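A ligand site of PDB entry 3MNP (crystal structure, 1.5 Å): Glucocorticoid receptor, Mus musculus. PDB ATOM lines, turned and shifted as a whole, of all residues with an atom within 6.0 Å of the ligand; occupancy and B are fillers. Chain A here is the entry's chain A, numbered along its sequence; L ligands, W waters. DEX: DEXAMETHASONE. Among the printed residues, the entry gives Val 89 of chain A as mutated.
The guanidinium group (NE) of Arg 95 is in hydrogen-bond range of the backbone carbonyl oxygen (O) of Cys 106 (3.0 Å).
NE2 of Gln 54 sits close to NH2 of Arg 95, at 3.5 Å.
The side-chain amide nitrogen of Gln 126 lies within hydrogen-bond range of the side-chain sulfur of Met 44, at 3.4 Å.
The backbone carbonyl oxygen (O) of Phe 107 lies within hydrogen-bond range of the guanidinium group (NH2) of Arg 95 (3.0 Å).
SD of Met 88 sits close to OE1 of Gln 54 (3.3 Å).
The backbone carbonyl oxygen (O) of Cys 220 is in hydrogen-bond range of the side-chain hydroxyl (OG1) of Thr 223, at 3.3 Å.
The side-chain amide nitrogen (ND2) of Asn 48 is in hydrogen-bond range of the backbone carbonyl oxygen (O) of Met 44, at 3.3 Å.
The side-chain hydroxyl of Thr 223 sits at hydrogen-bond distance from the backbone carbonyl oxygen of Tyr 219, 2.8 Å away.
The backbone carbonyl oxygen (O) of Tyr 219 lies close to an oxygen (O4) of the ligand (3.4 Å).
Met 44 touches the ligand.
O of Leu 47 touches C1 of the ligand (3.2 Å).
CA of Gly 51 touches C1 of the ligand, at 3.4 Å.
CZ3 of Trp 84 touches C19 of the ligand, at 3.8 Å.
SD of Met 85 touches C7 of the ligand, 3.8 Å away.
Met 88 touches the ligand.
Val 89 touches the ligand.
Phe 107 touches the ligand.
SD of Met 130 touches C14 of the ligand, at 3.8 Å.
Leu 216 touches the ligand.
Ile 231 touches the ligand.
Phe 233 touches the ligand.
Within 4 Å of the ligand: Met 44, Leu 47, Asn 48, Gly 51, Gln 54, Trp 84, Met 85, Met 88, Val 89, Arg 95, Phe 107, Gln 126, Met 130, Leu 216, Tyr 219, Cys 220, Thr 223, Ile 231 and Phe 233.
The nearest printed residue that does not touch the ligand is Leu 92 (4.1 Å).
The guanidinium group of Arg 95 lies within hydrogen-bond range of an oxygen (O1) of the ligand (2.8 Å).
The side-chain hydroxyl (OG1) of Thr 223 sits at hydrogen-bond distance from an oxygen (O5) of the ligand (2.9 Å).
The side-chain amide nitrogen of Gln 54 is in hydrogen-bond range of an oxygen (O1) of the ligand, at 2.7 Å.
An oxygen (O2) of the ligand is in hydrogen-bond range of the side-chain amide oxygen (OD1) of Asn 48 (2.8 Å).
The side-chain amide oxygen of Gln 126 sits at hydrogen-bond distance from an oxygen (O3) of the ligand, 2.8 Å away.
O4 of the ligand lies close to N of Cys 220 (3.3 Å).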
ATOM      1  N   MET A  44      16.274  -0.801 -29.801  1.00  0.00           N
ATOM      2  CA  MET A  44      16.620  -2.016 -30.556  1.00  0.00           C
ATOM      3  C   MET A  44      18.028  -1.938 -31.167  1.00  0.00           C
ATOM      4  O   MET A  44      18.799  -2.869 -31.042  1.00  0.00           O
ATOM      5  CB  MET A  44      15.544  -2.331 -31.600  1.00  0.00           C
ATOM      6  CG  MET A  44      14.253  -2.781 -30.929  1.00  0.00           C
ATOM      7  SD  MET A  44      13.012  -3.287 -32.238  1.00  0.00           S
ATOM      8  CE  MET A  44      12.200  -1.806 -32.545  1.00  0.00           C
ATOM      9  N   THR A  45      18.367  -0.817 -31.818  1.00  0.00           N
ATOM     10  CA  THR A  45      19.708  -0.670 -32.367  1.00  0.00           C
ATOM     11  C   THR A  45      20.762  -0.784 -31.251  1.00  0.00           C
ATOM     12  O   THR A  45      21.762  -1.483 -31.412  1.00  0.00           O
ATOM     13  CB  THR A  45      19.809   0.654 -33.109  1.00  0.00           C
ATOM     14  OG1 THR A  45      19.054   0.525 -34.310  1.00  0.00           O
ATOM     15  CG2 THR A  45      21.276   0.936 -33.466  1.00  0.00           C
ATOM     16  N   LEU A  47      20.598  -2.310 -28.411  1.00  0.00           N
ATOM     17  CA  LEU A  47      20.681  -3.692 -27.962  1.00  0.00           C
ATOM     18  C   LEU A  47      21.474  -4.530 -28.959  1.00  0.00           C
ATOM     19  O   LEU A  47      22.302  -5.377 -28.584  1.00  0.00           O
ATOM     20  CB  LEU A  47      19.299  -4.331 -27.742  1.00  0.00           C
ATOM     21  CG  LEU A  47      18.375  -3.601 -26.756  1.00  0.00           C
ATOM     22  CD1 LEU A  47      17.057  -4.401 -26.692  1.00  0.00           C
ATOM     23  CD2 LEU A  47      19.003  -3.479 -25.364  1.00  0.00           C
ATOM     24  N   ASN A  48      21.251  -4.314 -30.260  1.00  0.00           N
ATOM     25  CA  ASN A  48      22.014  -5.060 -31.233  1.00  0.00           C
ATOM     26  C   ASN A  48      23.528  -4.787 -31.188  1.00  0.00           C
ATOM     27  O   ASN A  48      24.338  -5.693 -31.371  1.00  0.00           O
ATOM     28  CB  ASN A  48      21.485  -4.820 -32.645  1.00  0.00           C
ATOM     29  CG  ASN A  48      20.122  -5.420 -32.857  1.00  0.00           C
ATOM     30  OD1 ASN A  48      19.826  -6.478 -32.335  1.00  0.00           O
ATOM     31  ND2 ASN A  48      19.311  -4.761 -33.688  1.00  0.00           N
ATOM     32  N   MET A  49      23.901  -3.524 -30.967  1.00  0.00           N
ATOM     33  CA  MET A  49      25.336  -3.176 -30.899  1.00  0.00           C
ATOM     34  C   MET A  49      25.961  -3.870 -29.654  1.00  0.00           C
ATOM     35  O   MET A  49      27.063  -4.400 -29.723  1.00  0.00           O
ATOM     36  CB  MET A  49      25.542  -1.656 -30.874  1.00  0.00           C
ATOM     37  CG  MET A  49      24.989  -0.951 -32.118  1.00  0.00           C
ATOM     38  SD  MET A  49      25.719  -1.560 -33.610  1.00  0.00           S
ATOM     39  CE  MET A  49      24.556  -0.958 -34.878  1.00  0.00           C
ATOM     40  N   LEU A  50      25.219  -3.890 -28.545  1.00  0.00           N
ATOM     41  CA  LEU A  50      25.714  -4.601 -27.354  1.00  0.00           C
ATOM     42  C   LEU A  50      25.811  -6.107 -27.664  1.00  0.00           C
ATOM     43  O   LEU A  50      26.795  -6.807 -27.326  1.00  0.00           O
ATOM     44  CB  LEU A  50      24.807  -4.352 -26.163  1.00  0.00           C
ATOM     45  CG  LEU A  50      25.061  -5.219 -24.930  1.00  0.00           C
ATOM     46  CD1 LEU A  50      26.486  -4.920 -24.378  1.00  0.00           C
ATOM     47  CD2 LEU A  50      23.961  -4.891 -23.917  1.00  0.00           C
ATOM     48  N   GLY A  51      24.765  -6.612 -28.318  1.00  0.00           N
ATOM     49  CA  GLY A  51      24.695  -8.013 -28.692  1.00  0.00           C
ATOM     50  C   GLY A  51      25.880  -8.457 -29.533  1.00  0.00           C
ATOM     51  O   GLY A  51      26.418  -9.545 -29.317  1.00  0.00           O
ATOM     52  N   GLY A  52      26.343  -7.628 -30.475  1.00  0.00           N
ATOM     53  CA  GLY A  52      27.459  -8.073 -31.296  1.00  0.00           C
ATOM     54  C   GLY A  52      28.717  -8.265 -30.447  1.00  0.00           C
ATOM     55  O   GLY A  52      29.477  -9.206 -30.648  1.00  0.00           O
ATOM     56  N   GLN A  54      28.708  -8.978 -27.246  1.00  0.00           N
ATOM     57  CA  GLN A  54      28.549 -10.176 -26.411  1.00  0.00           C
ATOM     58  C   GLN A  54      28.774 -11.457 -27.211  1.00  0.00           C
ATOM     59  O   GLN A  54      29.326 -12.435 -26.692  1.00  0.00           O
ATOM     60  CB  GLN A  54      27.154 -10.227 -25.793  1.00  0.00           C
ATOM     61  CG  GLN A  54      26.839  -9.111 -24.803  1.00  0.00           C
ATOM     62  CD  GLN A  54      25.364  -9.093 -24.450  1.00  0.00           C
ATOM     63  OE1 GLN A  54      24.574  -9.841 -25.038  1.00  0.00           O
ATOM     64  NE2 GLN A  54      24.978  -8.259 -23.491  1.00  0.00           N
ATOM     65  N   VAL A  55      28.363 -11.469 -28.481  1.00  0.00           N
ATOM     66  CA  VAL A  55      28.535 -12.637 -29.305  1.00  0.00           C
ATOM     67  C   VAL A  55      30.017 -12.905 -29.580  1.00  0.00           C
ATOM     68  O   VAL A  55      30.455 -14.038 -29.498  1.00  0.00           O
ATOM     69  CB  VAL A  55      27.671 -12.523 -30.597  1.00  0.00           C
ATOM     70  CG1 VAL A  55      28.033 -13.624 -31.619  1.00  0.00           C
ATOM     71  CG2 VAL A  55      26.170 -12.649 -30.216  1.00  0.00           C
ATOM     72  N   TRP A  84      23.618 -18.893 -30.828  1.00  0.00           N
ATOM     73  CA  TRP A  84      23.920 -17.569 -30.262  1.00  0.00           C
ATOM     74  C   TRP A  84      22.753 -16.889 -29.540  1.00  0.00           C
ATOM     75  O   TRP A  84      22.933 -16.354 -28.435  1.00  0.00           O
ATOM     76  CB  TRP A  84      24.556 -16.620 -31.315  1.00  0.00           C
ATOM     77  CG  TRP A  84      23.594 -16.057 -32.282  1.00  0.00           C
ATOM     78  CD1 TRP A  84      23.119 -16.688 -33.397  1.00  0.00           C
ATOM     79  CD2 TRP A  84      22.848 -14.828 -32.152  1.00  0.00           C
ATOM     80  NE1 TRP A  84      22.205 -15.872 -34.040  1.00  0.00           N
ATOM     81  CE2 TRP A  84      21.986 -14.755 -33.272  1.00  0.00           C
ATOM     82  CE3 TRP A  84      22.781 -13.835 -31.173  1.00  0.00           C
ATOM     83  CZ2 TRP A  84      21.081 -13.699 -33.446  1.00  0.00           C
ATOM     84  CZ3 TRP A  84      21.929 -12.733 -31.387  1.00  0.00           C
ATOM     85  CH2 TRP A  84      21.125 -12.669 -32.549  1.00  0.00           C
ATOM     86  N   MET A  85      21.557 -16.976 -30.102  1.00  0.00           N
ATOM     87  CA  MET A  85      20.426 -16.343 -29.429  1.00  0.00           C
ATOM     88  C   MET A  85      20.130 -17.013 -28.087  1.00  0.00           C
ATOM     89  O   MET A  85      19.747 -16.336 -27.117  1.00  0.00           O
ATOM     90  CB  MET A  85      19.158 -16.288 -30.347  1.00  0.00           C
ATOM     91  CG  MET A  85      17.950 -15.527 -29.736  1.00  0.00           C
ATOM     92  SD  MET A  85      18.216 -13.782 -29.518  1.00  0.00           S
ATOM     93  CE  MET A  85      17.991 -13.249 -31.310  1.00  0.00           C
ATOM     94  N   MET A  88      22.744 -15.709 -25.655  1.00  0.00           N
ATOM     95  CA  MET A  88      22.509 -14.307 -25.260  1.00  0.00           C
ATOM     96  C   MET A  88      21.296 -14.126 -24.361  1.00  0.00           C
ATOM     97  O   MET A  88      21.354 -13.368 -23.390  1.00  0.00           O
ATOM     98  CB  MET A  88      22.307 -13.425 -26.501  1.00  0.00           C
ATOM     99  CG  MET A  88      23.505 -13.428 -27.466  1.00  0.00           C
ATOM    100  SD  MET A  88      24.984 -12.769 -26.592  1.00  0.00           S
ATOM    101  CE  MET A  88      25.819 -14.154 -26.377  1.00  0.00           C
ATOM    102  N   VAL A  89      20.199 -14.810 -24.682  1.00  0.00           N
ATOM    103  CA  VAL A  89      18.983 -14.678 -23.879  1.00  0.00           C
ATOM    104  C   VAL A  89      19.147 -15.324 -22.520  1.00  0.00           C
ATOM    105  O   VAL A  89      18.637 -14.823 -21.514  1.00  0.00           O
ATOM    106  CB  VAL A  89      17.787 -15.276 -24.636  1.00  0.00           C
ATOM    107  CG1 VAL A  89      16.535 -15.294 -23.762  1.00  0.00           C
ATOM    108  CG2 VAL A  89      17.546 -14.461 -25.869  1.00  0.00           C
ATOM    109  N   LEU A  92      21.226 -12.961 -20.438  1.00  0.00           N
ATOM    110  CA  LEU A  92      20.386 -11.806 -20.105  1.00  0.00           C
ATOM    111  C   LEU A  92      19.423 -12.231 -18.961  1.00  0.00           C
ATOM    112  O   LEU A  92      19.163 -11.460 -18.012  1.00  0.00           O
ATOM    113  CB  LEU A  92      19.584 -11.438 -21.349  1.00  0.00           C
ATOM    114  CG  LEU A  92      18.440 -10.458 -21.114  1.00  0.00           C
ATOM    115  CD1 LEU A  92      18.976  -9.080 -20.625  1.00  0.00           C
ATOM    116  CD2 LEU A  92      17.643 -10.298 -22.419  1.00  0.00           C
ATOM    117  N   ARG A  95      21.491 -12.305 -15.609  1.00  0.00           N
ATOM    118  CA  ARG A  95      21.707 -10.932 -15.081  1.00  0.00           C
ATOM    119  C   ARG A  95      20.418 -10.361 -14.513  1.00  0.00           C
ATOM    120  O   ARG A  95      20.417  -9.752 -13.433  1.00  0.00           O
ATOM    121  CB  ARG A  95      22.273 -10.014 -16.161  1.00  0.00           C
ATOM    122  CG  ARG A  95      23.588 -10.477 -16.655  1.00  0.00           C
ATOM    123  CD  ARG A  95      24.205  -9.454 -17.594  1.00  0.00           C
ATOM    124  NE  ARG A  95      23.410  -9.157 -18.800  1.00  0.00           N
ATOM    125  CZ  ARG A  95      23.505  -9.795 -19.958  1.00  0.00           C
ATOM    126  NH1 ARG A  95      24.277 -10.884 -20.070  1.00  0.00           N
ATOM    127  NH2 ARG A  95      22.806  -9.362 -21.018  1.00  0.00           N
ATOM    128  N   CYS A 106      17.984  -6.591 -17.455  1.00  0.00           N
ATOM    129  CA  CYS A 106      19.333  -6.121 -17.158  1.00  0.00           C
ATOM    130  C   CYS A 106      20.322  -6.448 -18.270  1.00  0.00           C
ATOM    131  O   CYS A 106      21.064  -7.441 -18.212  1.00  0.00           O
ATOM    132  CB  CYS A 106      19.778  -6.696 -15.797  1.00  0.00           C
ATOM    133  SG  CYS A 106      18.668  -6.187 -14.458  1.00  0.00           S
ATOM    134  N   PHE A 107      20.297  -5.640 -19.319  1.00  0.00           N
ATOM    135  CA  PHE A 107      21.172  -5.907 -20.459  1.00  0.00           C
ATOM    136  C   PHE A 107      22.621  -5.735 -20.101  1.00  0.00           C
ATOM    137  O   PHE A 107      23.494  -6.482 -20.562  1.00  0.00           O
ATOM    138  CB  PHE A 107      20.788  -5.043 -21.684  1.00  0.00           C
ATOM    139  CG  PHE A 107      19.539  -5.502 -22.373  1.00  0.00           C
ATOM    140  CD1 PHE A 107      18.298  -4.996 -21.989  1.00  0.00           C
ATOM    141  CD2 PHE A 107      19.573  -6.530 -23.319  1.00  0.00           C
ATOM    142  CE1 PHE A 107      17.125  -5.417 -22.607  1.00  0.00           C
ATOM    143  CE2 PHE A 107      18.377  -6.967 -23.917  1.00  0.00           C
ATOM    144  CZ  PHE A 107      17.185  -6.419 -23.552  1.00  0.00           C
ATOM    145  N   GLN A 126       8.136  -7.853 -27.408  1.00  0.00           N
ATOM    146  CA  GLN A 126       9.479  -8.434 -27.414  1.00  0.00           C
ATOM    147  C   GLN A 126      10.077  -8.507 -26.012  1.00  0.00           C
ATOM    148  O   GLN A 126      10.760  -9.479 -25.659  1.00  0.00           O
ATOM    149  CB  GLN A 126      10.409  -7.702 -28.373  1.00  0.00           C
ATOM    150  CG  GLN A 126      10.680  -6.228 -28.049  1.00  0.00           C
ATOM    151  CD  GLN A 126      11.518  -5.581 -29.137  1.00  0.00           C
ATOM    152  OE1 GLN A 126      12.656  -5.976 -29.372  1.00  0.00           O
ATOM    153  NE2 GLN A 126      10.956  -4.583 -29.823  1.00  0.00           N
ATOM    154  N   MET A 130      11.703 -11.572 -23.949  1.00  0.00           N
ATOM    155  CA  MET A 130      13.095 -11.506 -23.453  1.00  0.00           C
ATOM    156  C   MET A 130      13.220 -11.732 -21.950  1.00  0.00           C
ATOM    157  O   MET A 130      14.252 -12.247 -21.489  1.00  0.00           O
ATOM    158  CB  MET A 130      13.752 -10.186 -23.818  1.00  0.00           C
ATOM    159  CG  MET A 130      14.018 -10.052 -25.301  1.00  0.00           C
ATOM    160  SD  MET A 130      15.053  -8.643 -25.758  1.00  0.00           S
ATOM    161  CE  MET A 130      13.820  -7.325 -25.762  1.00  0.00           C
ATOM    162  N   ASN A 215      10.385 -17.154 -30.595  1.00  0.00           N
ATOM    163  CA  ASN A 215       9.724 -15.847 -30.461  1.00  0.00           C
ATOM    164  C   ASN A 215      10.672 -14.701 -30.759  1.00  0.00           C
ATOM    165  O   ASN A 215      10.285 -13.681 -31.366  1.00  0.00           O
ATOM    166  CB  ASN A 215       9.136 -15.657 -29.064  1.00  0.00           C
ATOM    167  CG  ASN A 215       8.000 -16.645 -28.767  1.00  0.00           C
ATOM    168  OD1 ASN A 215       7.217 -16.970 -29.631  1.00  0.00           O
ATOM    169  ND2 ASN A 215       7.954 -17.146 -27.547  1.00  0.00           N
ATOM    170  N   LEU A 216      11.904 -14.844 -30.273  1.00  0.00           N
ATOM    171  CA  LEU A 216      12.909 -13.795 -30.427  1.00  0.00           C
ATOM    172  C   LEU A 216      13.551 -13.744 -31.808  1.00  0.00           C
ATOM    173  O   LEU A 216      13.841 -12.653 -32.299  1.00  0.00           O
ATOM    174  CB  LEU A 216      13.952 -13.945 -29.314  1.00  0.00           C
ATOM    175  CG  LEU A 216      13.295 -13.753 -27.943  1.00  0.00           C
ATOM    176  CD1 LEU A 216      14.296 -14.054 -26.816  1.00  0.00           C
ATOM    177  CD2 LEU A 216      12.572 -12.415 -27.764  1.00  0.00           C
ATOM    178  N   LEU A 217      13.794 -14.918 -32.425  1.00  0.00           N
ATOM    179  CA  LEU A 217      14.367 -14.893 -33.767  1.00  0.00           C
ATOM    180  C   LEU A 217      13.386 -14.231 -34.752  1.00  0.00           C
ATOM    181  O   LEU A 217      13.831 -13.625 -35.703  1.00  0.00           O
ATOM    182  CB  LEU A 217      14.678 -16.337 -34.242  1.00  0.00           C
ATOM    183  CG  LEU A 217      15.849 -16.987 -33.482  1.00  0.00           C
ATOM    184  CD1 LEU A 217      15.940 -18.461 -33.984  1.00  0.00           C
ATOM    185  CD2 LEU A 217      17.170 -16.217 -33.679  1.00  0.00           C
ATOM    186  N   TYR A 219      11.567 -11.637 -34.258  1.00  0.00           N
ATOM    187  CA  TYR A 219      11.933 -10.203 -34.233  1.00  0.00           C
ATOM    188  C   TYR A 219      13.302  -9.933 -34.836  1.00  0.00           C
ATOM    189  O   TYR A 219      13.494  -8.986 -35.605  1.00  0.00           O
ATOM    190  CB  TYR A 219      11.911  -9.680 -32.784  1.00  0.00           C
ATOM    191  CG  TYR A 219      10.539  -9.311 -32.346  1.00  0.00           C
ATOM    192  CD1 TYR A 219      10.012  -8.049 -32.673  1.00  0.00           C
ATOM    193  CD2 TYR A 219       9.718 -10.226 -31.721  1.00  0.00           C
ATOM    194  CE1 TYR A 219       8.737  -7.699 -32.260  1.00  0.00           C
ATOM    195  CE2 TYR A 219       8.423  -9.896 -31.297  1.00  0.00           C
ATOM    196  CZ  TYR A 219       7.941  -8.628 -31.599  1.00  0.00           C
ATOM    197  OH  TYR A 219       6.647  -8.298 -31.286  1.00  0.00           O
ATOM    198  N   CYS A 220      14.302 -10.728 -34.470  1.00  0.00           N
ATOM    199  CA  CYS A 220      15.637 -10.492 -34.928  1.00  0.00           C
ATOM    200  C   CYS A 220      15.684 -10.553 -36.448  1.00  0.00           C
ATOM    201  O   CYS A 220      16.224  -9.642 -37.098  1.00  0.00           O
ATOM    202  CB  CYS A 220      16.546 -11.587 -34.359  1.00  0.00           C
ATOM    203  SG  CYS A 220      18.240 -11.462 -34.891  1.00  0.00           S
ATOM    204  N   PHE A 221      15.097 -11.581 -37.020  1.00  0.00           N
ATOM    205  CA  PHE A 221      15.168 -11.724 -38.481  1.00  0.00           C
ATOM    206  C   PHE A 221      14.351 -10.653 -39.198  1.00  0.00           C
ATOM    207  O   PHE A 221      14.788 -10.177 -40.230  1.00  0.00           O
ATOM    208  CB  PHE A 221      14.686 -13.108 -38.891  1.00  0.00           C
ATOM    209  CG  PHE A 221      15.545 -14.250 -38.369  1.00  0.00           C
ATOM    210  CD1 PHE A 221      16.853 -14.034 -37.934  1.00  0.00           C
ATOM    211  CD2 PHE A 221      15.057 -15.532 -38.436  1.00  0.00           C
ATOM    212  CE1 PHE A 221      17.643 -15.098 -37.464  1.00  0.00           C
ATOM    213  CE2 PHE A 221      15.845 -16.616 -38.017  1.00  0.00           C
ATOM    214  CZ  PHE A 221      17.142 -16.379 -37.525  1.00  0.00           C
ATOM    215  N   THR A 223      13.509  -7.541 -38.159  1.00  0.00           N
ATOM    216  CA  THR A 223      14.156  -6.235 -38.030  1.00  0.00           C
ATOM    217  C   THR A 223      15.467  -6.181 -38.804  1.00  0.00           C
ATOM    218  O   THR A 223      15.910  -5.105 -39.221  1.00  0.00           O
ATOM    219  CB  THR A 223      14.334  -5.833 -36.543  1.00  0.00           C
ATOM    220  OG1 THR A 223      15.194  -6.800 -35.879  1.00  0.00           O
ATOM    221  CG2 THR A 223      12.988  -5.823 -35.815  1.00  0.00           C
ATOM    222  N   PHE A 224      16.120  -7.330 -38.974  1.00  0.00           N
ATOM    223  CA  PHE A 224      17.331  -7.371 -39.764  1.00  0.00           C
ATOM    224  C   PHE A 224      16.997  -7.215 -41.264  1.00  0.00           C
ATOM    225  O   PHE A 224      17.639  -6.440 -41.964  1.00  0.00           O
ATOM    226  CB  PHE A 224      18.044  -8.709 -39.610  1.00  0.00           C
ATOM    227  CG  PHE A 224      19.274  -8.811 -40.451  1.00  0.00           C
ATOM    228  CD1 PHE A 224      20.355  -7.983 -40.197  1.00  0.00           C
ATOM    229  CD2 PHE A 224      19.285  -9.612 -41.584  1.00  0.00           C
ATOM    230  CE1 PHE A 224      21.463  -7.998 -41.024  1.00  0.00           C
ATOM    231  CE2 PHE A 224      20.419  -9.678 -42.383  1.00  0.00           C
ATOM    232  CZ  PHE A 224      21.503  -8.841 -42.109  1.00  0.00           C
ATOM    233  N   ILE A 231      16.747  -0.326 -38.309  1.00  0.00           N
ATOM    234  CA  ILE A 231      17.299  -0.891 -37.068  1.00  0.00           C
ATOM    235  C   ILE A 231      18.610  -1.442 -37.511  1.00  0.00           C
ATOM    236  O   ILE A 231      18.660  -2.214 -38.472  1.00  0.00           O
ATOM    237  CB  ILE A 231      16.383  -1.975 -36.488  1.00  0.00           C
ATOM    238  CG1 ILE A 231      15.121  -1.312 -35.942  1.00  0.00           C
ATOM    239  CG2 ILE A 231      17.096  -2.758 -35.359  1.00  0.00           C
ATOM    240  CD1 ILE A 231      13.995  -2.320 -35.701  1.00  0.00           C
ATOM    241  N   PHE A 233      22.445  -3.378 -37.098  1.00  0.00           N
ATOM    242  CA  PHE A 233      23.118  -4.522 -36.489  1.00  0.00           C
ATOM    243  C   PHE A 233      24.623  -4.382 -36.783  1.00  0.00           C
ATOM    244  O   PHE A 233      25.025  -3.985 -37.890  1.00  0.00           O
ATOM    245  CB  PHE A 233      22.651  -5.798 -37.154  1.00  0.00           C
ATOM    246  CG  PHE A 233      21.249  -6.210 -36.762  1.00  0.00           C
ATOM    247  CD1 PHE A 233      20.150  -5.588 -37.341  1.00  0.00           C
ATOM    248  CD2 PHE A 233      21.044  -7.222 -35.852  1.00  0.00           C
ATOM    249  CE1 PHE A 233      18.875  -5.982 -37.030  1.00  0.00           C
ATOM    250  CE2 PHE A 233      19.732  -7.623 -35.519  1.00  0.00           C
ATOM    251  CZ  PHE A 233      18.669  -6.994 -36.120  1.00  0.00           C
ATOM    252  N   LEU A 237      27.165  -9.713 -36.000  1.00  0.00           N
ATOM    253  CA  LEU A 237      25.791 -10.201 -35.896  1.00  0.00           C
ATOM    254  C   LEU A 237      25.146 -10.283 -37.263  1.00  0.00           C
ATOM    255  O   LEU A 237      24.457 -11.253 -37.568  1.00  0.00           O
ATOM    256  CB  LEU A 237      24.978  -9.305 -34.993  1.00  0.00           C
ATOM    257  CG  LEU A 237      24.278  -9.911 -33.790  1.00  0.00           C
ATOM    258  CD1 LEU A 237      25.230 -10.728 -32.942  1.00  0.00           C
ATOM    259  CD2 LEU A 237      23.613  -8.830 -32.963  1.00  0.00           C
HETATM  260  C1  DEX L   1      21.612  -8.174 -27.174  1.00  0.00           C
HETATM  261  C2  DEX L   1      22.115  -8.160 -25.960  1.00  0.00           C
HETATM  262  C3  DEX L   1      21.841  -9.065 -24.865  1.00  0.00           C
HETATM  263  C4  DEX L   1      20.854 -10.155 -25.072  1.00  0.00           C
HETATM  264  C5  DEX L   1      20.300 -10.258 -26.330  1.00  0.00           C
HETATM  265  C6  DEX L   1      19.255 -11.343 -26.560  1.00  0.00           C
HETATM  266  C7  DEX L   1      17.934 -10.806 -27.114  1.00  0.00           C
HETATM  267  C8  DEX L   1      18.254  -9.895 -28.485  1.00  0.00           C
HETATM  268  C9  DEX L   1      19.307  -8.747 -28.072  1.00  0.00           C
HETATM  269  C10 DEX L   1      20.669  -9.404 -27.450  1.00  0.00           C
HETATM  270  C11 DEX L   1      19.513  -7.709 -29.192  1.00  0.00           C
HETATM  271  C12 DEX L   1      18.134  -7.219 -29.763  1.00  0.00           C
HETATM  272  C13 DEX L   1      17.238  -8.439 -30.249  1.00  0.00           C
HETATM  273  C14 DEX L   1      16.954  -9.308 -29.003  1.00  0.00           C
HETATM  274  C15 DEX L   1      15.788 -10.278 -29.396  1.00  0.00           C
HETATM  275  C16 DEX L   1      14.989  -9.363 -30.378  1.00  0.00           C
HETATM  276  C17 DEX L   1      15.699  -8.013 -30.543  1.00  0.00           C
HETATM  277  C18 DEX L   1      17.875  -9.155 -31.515  1.00  0.00           C
HETATM  278  C19 DEX L   1      21.379 -10.315 -28.465  1.00  0.00           C
HETATM  279  C20 DEX L   1      15.543  -7.449 -31.894  1.00  0.00           C
HETATM  280  C21 DEX L   1      15.846  -5.975 -32.130  1.00  0.00           C
HETATM  281  C22 DEX L   1      13.537  -9.156 -29.746  1.00  0.00           C
HETATM  282  F1  DEX L   1      18.723  -8.081 -27.061  1.00  0.00           F
HETATM  283  O1  DEX L   1      22.359  -8.915 -23.748  1.00  0.00           O
HETATM  284  O2  DEX L   1      20.337  -8.262 -30.243  1.00  0.00           O
HETATM  285  O3  DEX L   1      15.292  -7.007 -29.583  1.00  0.00           O
HETATM  286  O4  DEX L   1      15.295  -8.055 -32.855  1.00  0.00           O
HETATM  287  O5  DEX L   1      16.201  -5.608 -33.492  1.00  0.00           O
HETATM  288  O   HOH W   1      23.607 -11.644 -22.962  1.00  0.00           O
